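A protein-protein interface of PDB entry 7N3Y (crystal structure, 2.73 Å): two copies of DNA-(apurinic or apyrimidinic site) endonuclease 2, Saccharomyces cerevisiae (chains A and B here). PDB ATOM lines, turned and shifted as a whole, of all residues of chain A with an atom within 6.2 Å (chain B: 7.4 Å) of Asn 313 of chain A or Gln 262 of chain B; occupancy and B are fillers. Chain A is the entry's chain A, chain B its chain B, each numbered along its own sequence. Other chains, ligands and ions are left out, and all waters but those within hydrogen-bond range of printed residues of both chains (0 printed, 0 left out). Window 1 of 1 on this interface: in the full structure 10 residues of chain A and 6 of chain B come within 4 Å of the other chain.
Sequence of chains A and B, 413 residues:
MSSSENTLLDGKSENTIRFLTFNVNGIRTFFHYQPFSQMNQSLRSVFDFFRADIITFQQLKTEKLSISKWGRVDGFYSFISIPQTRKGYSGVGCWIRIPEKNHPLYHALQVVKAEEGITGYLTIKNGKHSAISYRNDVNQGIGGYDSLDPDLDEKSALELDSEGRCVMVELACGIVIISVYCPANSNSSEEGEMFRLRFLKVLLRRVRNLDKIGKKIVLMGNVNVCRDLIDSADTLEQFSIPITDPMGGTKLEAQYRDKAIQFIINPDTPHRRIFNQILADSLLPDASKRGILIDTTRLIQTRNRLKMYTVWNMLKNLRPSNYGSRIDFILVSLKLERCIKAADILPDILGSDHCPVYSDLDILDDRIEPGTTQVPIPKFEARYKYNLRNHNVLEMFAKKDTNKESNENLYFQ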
ATOM      1  N   VAL A 311      22.956  -1.519  24.456  1.00  0.00           N
ATOM      2  CA  VAL A 311      24.078  -2.100  23.724  1.00  0.00           C
ATOM      3  C   VAL A 311      23.644  -2.377  22.291  1.00  0.00           C
ATOM      4  O   VAL A 311      22.521  -2.829  22.044  1.00  0.00           O
ATOM      5  CB  VAL A 311      24.604  -3.388  24.399  1.00  0.00           C
ATOM      6  CG1 VAL A 311      23.501  -4.432  24.529  1.00  0.00           C
ATOM      7  CG2 VAL A 311      25.789  -3.956  23.626  1.00  0.00           C
ATOM      8  N   TRP A 312      24.534  -2.081  21.342  1.00  0.00           N
ATOM      9  CA  TRP A 312      24.367  -2.411  19.926  1.00  0.00           C
ATOM     10  C   TRP A 312      25.693  -3.036  19.505  1.00  0.00           C
ATOM     11  O   TRP A 312      26.606  -2.324  19.078  1.00  0.00           O
ATOM     12  CB  TRP A 312      24.020  -1.180  19.093  1.00  0.00           C
ATOM     13  CG  TRP A 312      22.812  -0.460  19.592  1.00  0.00           C
ATOM     14  CD1 TRP A 312      21.540  -0.553  19.105  1.00  0.00           C
ATOM     15  CD2 TRP A 312      22.757   0.454  20.691  1.00  0.00           C
ATOM     16  NE1 TRP A 312      20.698   0.252  19.831  1.00  0.00           N
ATOM     17  CE2 TRP A 312      21.421   0.882  20.811  1.00  0.00           C
ATOM     18  CE3 TRP A 312      23.708   0.954  21.587  1.00  0.00           C
ATOM     19  CZ2 TRP A 312      21.013   1.784  21.789  1.00  0.00           C
ATOM     20  CZ3 TRP A 312      23.300   1.849  22.555  1.00  0.00           C
ATOM     21  CH2 TRP A 312      21.966   2.256  22.648  1.00  0.00           C
ATOM     22  N   ASN A 313      25.780  -4.361  19.625  1.00  0.00           N
ATOM     23  CA  ASN A 313      27.060  -5.064  19.600  1.00  0.00           C
ATOM     24  C   ASN A 313      27.892  -4.687  18.381  1.00  0.00           C
ATOM     25  O   ASN A 313      27.420  -4.753  17.244  1.00  0.00           O
ATOM     26  CB  ASN A 313      26.819  -6.575  19.627  1.00  0.00           C
ATOM     27  CG  ASN A 313      28.092  -7.363  19.860  1.00  0.00           C
ATOM     28  OD1 ASN A 313      29.078  -6.834  20.372  1.00  0.00           O
ATOM     29  ND2 ASN A 313      28.078  -8.638  19.486  1.00  0.00           N
ATOM     30  N   MET A 314      29.132  -4.267  18.640  1.00  0.00           N
ATOM     31  CA  MET A 314      30.172  -3.950  17.663  1.00  0.00           C
ATOM     32  C   MET A 314      29.940  -2.638  16.922  1.00  0.00           C
ATOM     33  O   MET A 314      30.739  -2.298  16.046  1.00  0.00           O
ATOM     34  CB  MET A 314      30.358  -5.071  16.628  1.00  0.00           C
ATOM     35  CG  MET A 314      30.706  -6.414  17.237  1.00  0.00           C
ATOM     36  SD  MET A 314      30.774  -7.756  16.036  1.00  0.00           S
ATOM     37  CE  MET A 314      31.150  -9.136  17.113  1.00  0.00           C
ATOM     38  N   LEU A 315      28.888  -1.888  17.240  1.00  0.00           N
ATOM     39  CA  LEU A 315      28.559  -0.651  16.536  1.00  0.00           C
ATOM     40  C   LEU A 315      28.750   0.524  17.487  1.00  0.00           C
ATOM     41  O   LEU A 315      27.990   0.684  18.447  1.00  0.00           O
ATOM     42  CB  LEU A 315      27.132  -0.698  15.996  1.00  0.00           C
ATOM     43  CG  LEU A 315      26.885  -1.750  14.911  1.00  0.00           C
ATOM     44  CD1 LEU A 315      25.430  -1.747  14.471  1.00  0.00           C
ATOM     45  CD2 LEU A 315      27.809  -1.528  13.723  1.00  0.00           C
ATOM     46  N   TYR A 323      17.488  -3.705  16.499  1.00  0.00           N
ATOM     47  CA  TYR A 323      18.797  -4.232  16.854  1.00  0.00           C
ATOM     48  C   TYR A 323      19.201  -3.654  18.201  1.00  0.00           C
ATOM     49  O   TYR A 323      19.001  -2.463  18.452  1.00  0.00           O
ATOM     50  CB  TYR A 323      19.833  -3.885  15.778  1.00  0.00           C
ATOM     51  CG  TYR A 323      21.231  -4.387  16.052  1.00  0.00           C
ATOM     52  CD1 TYR A 323      21.517  -5.746  16.033  1.00  0.00           C
ATOM     53  CD2 TYR A 323      22.271  -3.502  16.307  1.00  0.00           C
ATOM     54  CE1 TYR A 323      22.795  -6.209  16.279  1.00  0.00           C
ATOM     55  CE2 TYR A 323      23.555  -3.955  16.550  1.00  0.00           C
ATOM     56  CZ  TYR A 323      23.811  -5.310  16.533  1.00  0.00           C
ATOM     57  OH  TYR A 323      25.086  -5.767  16.776  1.00  0.00           O
ATOM     58  N   GLY A 324      19.751  -4.499  19.062  1.00  0.00           N
ATOM     59  CA  GLY A 324      20.261  -4.072  20.348  1.00  0.00           C
ATOM     60  C   GLY A 324      19.584  -4.780  21.509  1.00  0.00           C
ATOM     61  O   GLY A 324      18.615  -5.521  21.354  1.00  0.00           O
ATOM     62  N   ASP A 353      29.954   0.612  21.766  1.00  0.00           N
ATOM     63  CA  ASP A 353      28.754  -0.129  21.407  1.00  0.00           C
ATOM     64  C   ASP A 353      27.729  -0.142  22.533  1.00  0.00           C
ATOM     65  O   ASP A 353      26.615  -0.638  22.335  1.00  0.00           O
ATOM     66  CB  ASP A 353      29.108  -1.559  20.979  1.00  0.00           C
ATOM     67  CG  ASP A 353      30.026  -2.256  21.958  1.00  0.00           C
ATOM     68  OD1 ASP A 353      30.673  -1.563  22.769  1.00  0.00           O
ATOM     69  OD2 ASP A 353      30.108  -3.501  21.903  1.00  0.00           O
ATOM     70  N   PHE B 239      27.284 -21.011  16.546  1.00  0.00           N
ATOM     71  CA  PHE B 239      26.052 -20.249  16.697  1.00  0.00           C
ATOM     72  C   PHE B 239      24.808 -21.125  16.650  1.00  0.00           C
ATOM     73  O   PHE B 239      23.695 -20.591  16.705  1.00  0.00           O
ATOM     74  CB  PHE B 239      25.958 -19.174  15.608  1.00  0.00           C
ATOM     75  CG  PHE B 239      27.052 -18.143  15.670  1.00  0.00           C
ATOM     76  CD1 PHE B 239      27.772 -17.937  16.836  1.00  0.00           C
ATOM     77  CD2 PHE B 239      27.356 -17.372  14.558  1.00  0.00           C
ATOM     78  CE1 PHE B 239      28.775 -16.988  16.890  1.00  0.00           C
ATOM     79  CE2 PHE B 239      28.356 -16.420  14.608  1.00  0.00           C
ATOM     80  CZ  PHE B 239      29.069 -16.230  15.776  1.00  0.00           C
ATOM     81  N   TYR B 256      19.504 -14.882  10.206  1.00  0.00           N
ATOM     82  CA  TYR B 256      20.659 -14.613  11.054  1.00  0.00           C
ATOM     83  C   TYR B 256      21.471 -13.437  10.519  1.00  0.00           C
ATOM     84  O   TYR B 256      22.702 -13.485  10.454  1.00  0.00           O
ATOM     85  CB  TYR B 256      21.529 -15.860  11.188  1.00  0.00           C
ATOM     86  CG  TYR B 256      20.784 -17.039  11.768  1.00  0.00           C
ATOM     87  CD1 TYR B 256      20.723 -17.239  13.141  1.00  0.00           C
ATOM     88  CD2 TYR B 256      20.130 -17.946  10.945  1.00  0.00           C
ATOM     89  CE1 TYR B 256      20.038 -18.313  13.678  1.00  0.00           C
ATOM     90  CE2 TYR B 256      19.442 -19.023  11.473  1.00  0.00           C
ATOM     91  CZ  TYR B 256      19.399 -19.203  12.839  1.00  0.00           C
ATOM     92  OH  TYR B 256      18.715 -20.272  13.371  1.00  0.00           O
ATOM     93  N   ARG B 257      20.772 -12.364  10.137  1.00  0.00           N
ATOM     94  CA  ARG B 257      21.436 -11.175   9.612  1.00  0.00           C
ATOM     95  C   ARG B 257      22.418 -10.590  10.619  1.00  0.00           C
ATOM     96  O   ARG B 257      23.482 -10.086  10.240  1.00  0.00           O
ATOM     97  CB  ARG B 257      20.388 -10.135   9.217  1.00  0.00           C
ATOM     98  CG  ARG B 257      20.944  -8.759   8.897  1.00  0.00           C
ATOM     99  CD  ARG B 257      19.855  -7.704   9.011  1.00  0.00           C
ATOM    100  NE  ARG B 257      19.187  -7.767  10.308  1.00  0.00           N
ATOM    101  CZ  ARG B 257      18.222  -6.940  10.696  1.00  0.00           C
ATOM    102  NH1 ARG B 257      17.806  -5.976   9.885  1.00  0.00           N
ATOM    103  NH2 ARG B 257      17.674  -7.078  11.895  1.00  0.00           N
ATOM    104  N   ASP B 258      22.081 -10.651  11.910  1.00  0.00           N
ATOM    105  CA  ASP B 258      22.962 -10.097  12.932  1.00  0.00           C
ATOM    106  C   ASP B 258      24.295 -10.837  12.967  1.00  0.00           C
ATOM    107  O   ASP B 258      25.364 -10.219  12.909  1.00  0.00           O
ATOM    108  CB  ASP B 258      22.276 -10.143  14.298  1.00  0.00           C
ATOM    109  CG  ASP B 258      21.083  -9.204  14.388  1.00  0.00           C
ATOM    110  OD1 ASP B 258      20.832  -8.458  13.416  1.00  0.00           O
ATOM    111  OD2 ASP B 258      20.395  -9.213  15.433  1.00  0.00           O
ATOM    112  N   LYS B 259      24.250 -12.169  13.050  1.00  0.00           N
ATOM    113  CA  LYS B 259      25.485 -12.946  13.091  1.00  0.00           C
ATOM    114  C   LYS B 259      26.272 -12.822  11.791  1.00  0.00           C
ATOM    115  O   LYS B 259      27.505 -12.898  11.809  1.00  0.00           O
ATOM    116  CB  LYS B 259      25.175 -14.414  13.390  1.00  0.00           C
ATOM    117  CG  LYS B 259      24.605 -14.668  14.782  1.00  0.00           C
ATOM    118  CD  LYS B 259      25.638 -14.388  15.865  1.00  0.00           C
ATOM    119  CE  LYS B 259      25.046 -14.527  17.261  1.00  0.00           C
ATOM    120  NZ  LYS B 259      24.010 -13.487  17.539  1.00  0.00           N
ATOM    121  N   ALA B 260      25.584 -12.619  10.663  1.00  0.00           N
ATOM    122  CA  ALA B 260      26.279 -12.499   9.383  1.00  0.00           C
ATOM    123  C   ALA B 260      27.062 -11.194   9.296  1.00  0.00           C
ATOM    124  O   ALA B 260      28.159 -11.159   8.723  1.00  0.00           O
ATOM    125  CB  ALA B 260      25.282 -12.600   8.229  1.00  0.00           C
ATOM    126  N   ILE B 261      26.515 -10.110   9.848  1.00  0.00           N
ATOM    127  CA  ILE B 261      27.221  -8.835   9.825  1.00  0.00           C
ATOM    128  C   ILE B 261      28.266  -8.782  10.930  1.00  0.00           C
ATOM    129  O   ILE B 261      29.399  -8.343  10.703  1.00  0.00           O
ATOM    130  CB  ILE B 261      26.222  -7.667   9.927  1.00  0.00           C
ATOM    131  CG1 ILE B 261      25.293  -7.662   8.716  1.00  0.00           C
ATOM    132  CG2 ILE B 261      26.959  -6.342  10.010  1.00  0.00           C
ATOM    133  CD1 ILE B 261      26.021  -7.458   7.403  1.00  0.00           C
ATOM    134  N   GLN B 262      27.911  -9.231  12.139  1.00  0.00           N
ATOM    135  CA  GLN B 262      28.893  -9.287  13.220  1.00  0.00           C
ATOM    136  C   GLN B 262      30.081 -10.166  12.852  1.00  0.00           C
ATOM    137  O   GLN B 262      31.186  -9.968  13.371  1.00  0.00           O
ATOM    138  CB  GLN B 262      28.239  -9.797  14.504  1.00  0.00           C
ATOM    139  CG  GLN B 262      27.207  -8.852  15.086  1.00  0.00           C
ATOM    140  CD  GLN B 262      26.383  -9.497  16.180  1.00  0.00           C
ATOM    141  OE1 GLN B 262      26.516 -10.691  16.456  1.00  0.00           O
ATOM    142  NE2 GLN B 262      25.524  -8.707  16.811  1.00  0.00           N
ATOM    143  N   PHE B 263      29.872 -11.138  11.960  1.00  0.00           N
ATOM    144  CA  PHE B 263      30.972 -11.968  11.482  1.00  0.00           C
ATOM    145  C   PHE B 263      32.000 -11.152  10.713  1.00  0.00           C
ATOM    146  O   PHE B 263      33.197 -11.449  10.768  1.00  0.00           O
ATOM    147  CB  PHE B 263      30.432 -13.087  10.595  1.00  0.00           C
ATOM    148  CG  PHE B 263      31.417 -14.188  10.341  1.00  0.00           C
ATOM    149  CD1 PHE B 263      31.531 -15.242  11.229  1.00  0.00           C
ATOM    150  CD2 PHE B 263      32.229 -14.171   9.218  1.00  0.00           C
ATOM    151  CE1 PHE B 263      32.434 -16.261  11.005  1.00  0.00           C
ATOM    152  CE2 PHE B 263      33.136 -15.191   8.989  1.00  0.00           C
ATOM    153  CZ  PHE B 263      33.235 -16.237   9.884  1.00  0.00           C
ATOM    154  N   ILE B 264      31.552 -10.127   9.990  1.00  0.00           N
ATOM    155  CA  ILE B 264      32.447  -9.359   9.132  1.00  0.00           C
ATOM    156  C   ILE B 264      33.204  -8.310   9.935  1.00  0.00           C
ATOM    157  O   ILE B 264      34.418  -8.140   9.772  1.00  0.00           O
ATOM    158  CB  ILE B 264      31.650  -8.719   7.983  1.00  0.00           C
ATOM    159  CG1 ILE B 264      31.058  -9.796   7.074  1.00  0.00           C
ATOM    160  CG2 ILE B 264      32.520  -7.757   7.195  1.00  0.00           C
ATOM    161  CD1 ILE B 264      30.189  -9.242   5.977  1.00  0.00           C
ATOM    162  N   ILE B 265      32.504  -7.590  10.813  1.00  0.00           N
ATOM    163  CA  ILE B 265      33.069  -6.423  11.478  1.00  0.00           C
ATOM    164  C   ILE B 265      33.632  -6.759  12.857  1.00  0.00           C
ATOM    165  O   ILE B 265      34.047  -5.852  13.583  1.00  0.00           O
ATOM    166  CB  ILE B 265      32.034  -5.290  11.577  1.00  0.00           C
ATOM    167  CG1 ILE B 265      30.896  -5.675  12.520  1.00  0.00           C
ATOM    168  CG2 ILE B 265      31.476  -4.948  10.203  1.00  0.00           C
ATOM    169  CD1 ILE B 265      29.943  -4.535  12.794  1.00  0.00           C
ATOM    170  N   ASN B 266      33.669  -8.035  13.227  1.00  0.00           N
ATOM    171  CA  ASN B 266      34.138  -8.446  14.546  1.00  0.00           C
ATOM    172  C   ASN B 266      35.557  -7.947  14.797  1.00  0.00           C
ATOM    173  O   ASN B 266      36.487  -8.370  14.093  1.00  0.00           O
ATOM    174  CB  ASN B 266      34.089  -9.968  14.667  1.00  0.00           C
ATOM    175  CG  ASN B 266      34.239 -10.452  16.100  1.00  0.00           C
ATOM    176  OD1 ASN B 266      34.886  -9.809  16.930  1.00  0.00           O
ATOM    177  ND2 ASN B 266      33.631 -11.596  16.397  1.00  0.00           N
ATOM    178  N   PRO B 267      35.775  -7.072  15.784  1.00  0.00           N
ATOM    179  CA  PRO B 267      37.141  -6.587  16.043  1.00  0.00           C
ATOM    180  C   PRO B 267      38.083  -7.659  16.565  1.00  0.00           C
ATOM    181  O   PRO B 267      39.302  -7.462  16.503  1.00  0.00           O
ATOM    182  CB  PRO B 267      36.930  -5.476  17.081  1.00  0.00           C
ATOM    183  CG  PRO B 267      35.662  -5.851  17.770  1.00  0.00           C
ATOM    184  CD  PRO B 267      34.793  -6.485  16.713  1.00  0.00           C
ATOM    185  N   THR B 269      38.437 -10.547  15.180  1.00  0.00           N
ATOM    186  CA  THR B 269      38.925 -11.235  13.984  1.00  0.00           C
ATOM    187  C   THR B 269      39.145 -10.217  12.868  1.00  0.00           C
ATOM    188  O   THR B 269      38.491 -10.270  11.822  1.00  0.00           O
ATOM    189  CB  THR B 269      37.941 -12.320  13.547  1.00  0.00           C
ATOM    190  OG1 THR B 269      36.687 -11.719  13.191  1.00  0.00           O
ATOM    191  CG2 THR B 269      37.711 -13.323  14.667  1.00  0.00           C
ATOM    192  N   ARG B 272      39.173 -10.740   8.958  1.00  0.00           N
ATOM    193  CA  ARG B 272      37.928 -10.889   8.212  1.00  0.00           C
ATOM    194  C   ARG B 272      37.364  -9.540   7.787  1.00  0.00           C
ATOM    195  O   ARG B 272      36.722  -9.444   6.735  1.00  0.00           O
ATOM    196  CB  ARG B 272      36.910 -11.660   9.049  1.00  0.00           C
ATOM    197  CG  ARG B 272      37.369 -13.063   9.402  1.00  0.00           C
ATOM    198  CD  ARG B 272      36.428 -13.753  10.376  1.00  0.00           C
ATOM    199  NE  ARG B 272      36.748 -15.173  10.498  1.00  0.00           N
ATOM    200  CZ  ARG B 272      36.212 -15.990  11.397  1.00  0.00           C
ATOM    201  NH1 ARG B 272      35.324 -15.530  12.267  1.00  0.00           N
ATOM    202  NH2 ARG B 272      36.565 -17.268  11.425  1.00  0.00           N
ATOM    203  N   LEU B 284      28.322  -5.612   3.431  1.00  0.00           N
ATOM    204  CA  LEU B 284      28.137  -4.309   4.042  1.00  0.00           C
ATOM    205  C   LEU B 284      27.472  -3.342   3.062  1.00  0.00           C
ATOM    206  O   LEU B 284      27.619  -3.478   1.845  1.00  0.00           O
ATOM    207  CB  LEU B 284      29.479  -3.756   4.512  1.00  0.00           C
ATOM    208  CG  LEU B 284      30.085  -4.527   5.686  1.00  0.00           C
ATOM    209  CD1 LEU B 284      31.352  -3.852   6.171  1.00  0.00           C
ATOM    210  CD2 LEU B 284      29.078  -4.651   6.817  1.00  0.00           C
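No position is printed for both chains.
The backbone carbonyl oxygen (O) of Tyr 323 of chain A lies close to the indole nitrogen (NE1) of Trp 312 of chain A (3.5 Å).
O of Asn 313 of chain A lies within hydrogen-bond range of OH of Tyr 323 of chain A (2.6 Å).
N of Met 314 of chain A lies within hydrogen-bond range of OD2 of Asp 353 of chain A, 3.5 Å away.
The guanidinium group of Arg 257 of chain B is in salt-bridge range of the side-chain carboxylate of Asp 258 of chain B, 3.6 Å away.
The backbone carbonyl oxygen (O) of Asn 266 of chain B lies close to the side-chain hydroxyl (OG1) of Thr 269 of chain B (3.5 Å).
Among the printed residues, pairs that only touch across the chains: Asn 313 of chain A with Gln 262 of chain B (3.7 Å), Met 314 of chain A with Ile 265 of chain B (3.9 Å), Met 314 of chain A with Asn 266 of chain B (3.5 Å), Leu 315 of chain A with Ile 265 of chain B (3.8 Å) and Tyr 323 of chain A with Asp 258 of chain B (3.7 Å).
The side-chain hydroxyl (OH) of Tyr 323 of chain A lies within hydrogen-bond range of the side-chain amide nitrogen (NE2) of Gln 262 of chain B, 3.0 Å away.
The backbone carbonyl oxygen (O) of Gln 262 of chain B lies close to the side-chain sulfur (SD) of Met 314 of chain A.
Hydrophobic or aromatic side chains of chain B that line the printed part of chain A: Ile 265.
Among the printed residues, no Asp or Glu carboxylate lies within 4 Å of a Lys or Arg side-chain nitrogen of the other chain.
Asn 313 of chain A touches one residue of chain B.
Printed residues of chain B within 4 Å of Met 314 of chain A: Gln 262 (3.5 Å), Ile 265 (3.9 Å) and Asn 266 (3.5 Å).
Of the printed residues of chain B, Leu 315 of chain A touches Ile 265.
Printed residues of chain B within 4 Å of Tyr 323 of chain A: Asp 258 (3.7 Å) and Gln 262 (3.0 Å).
Ile 261 of chain B touches none of the printed residues of chain A.
Of chain A, only Asn 313 (3.7 Å), Met 314 (3.5 Å) and Tyr 323 (3.0 Å) come within 4 Å of Gln 262 of chain B.
Of the printed residues of chain A, Ile 265 of chain B touches Met 314 and Leu 315.
Of the printed residues of chain A, Asn 266 of chain B touches Met 314.
Leu 284 of chain B touches none of the printed residues of chain A.
The nearest residue of chain B that does not touch Asn 313 of chain A is Ile 265 of chain B (5.1 Å).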
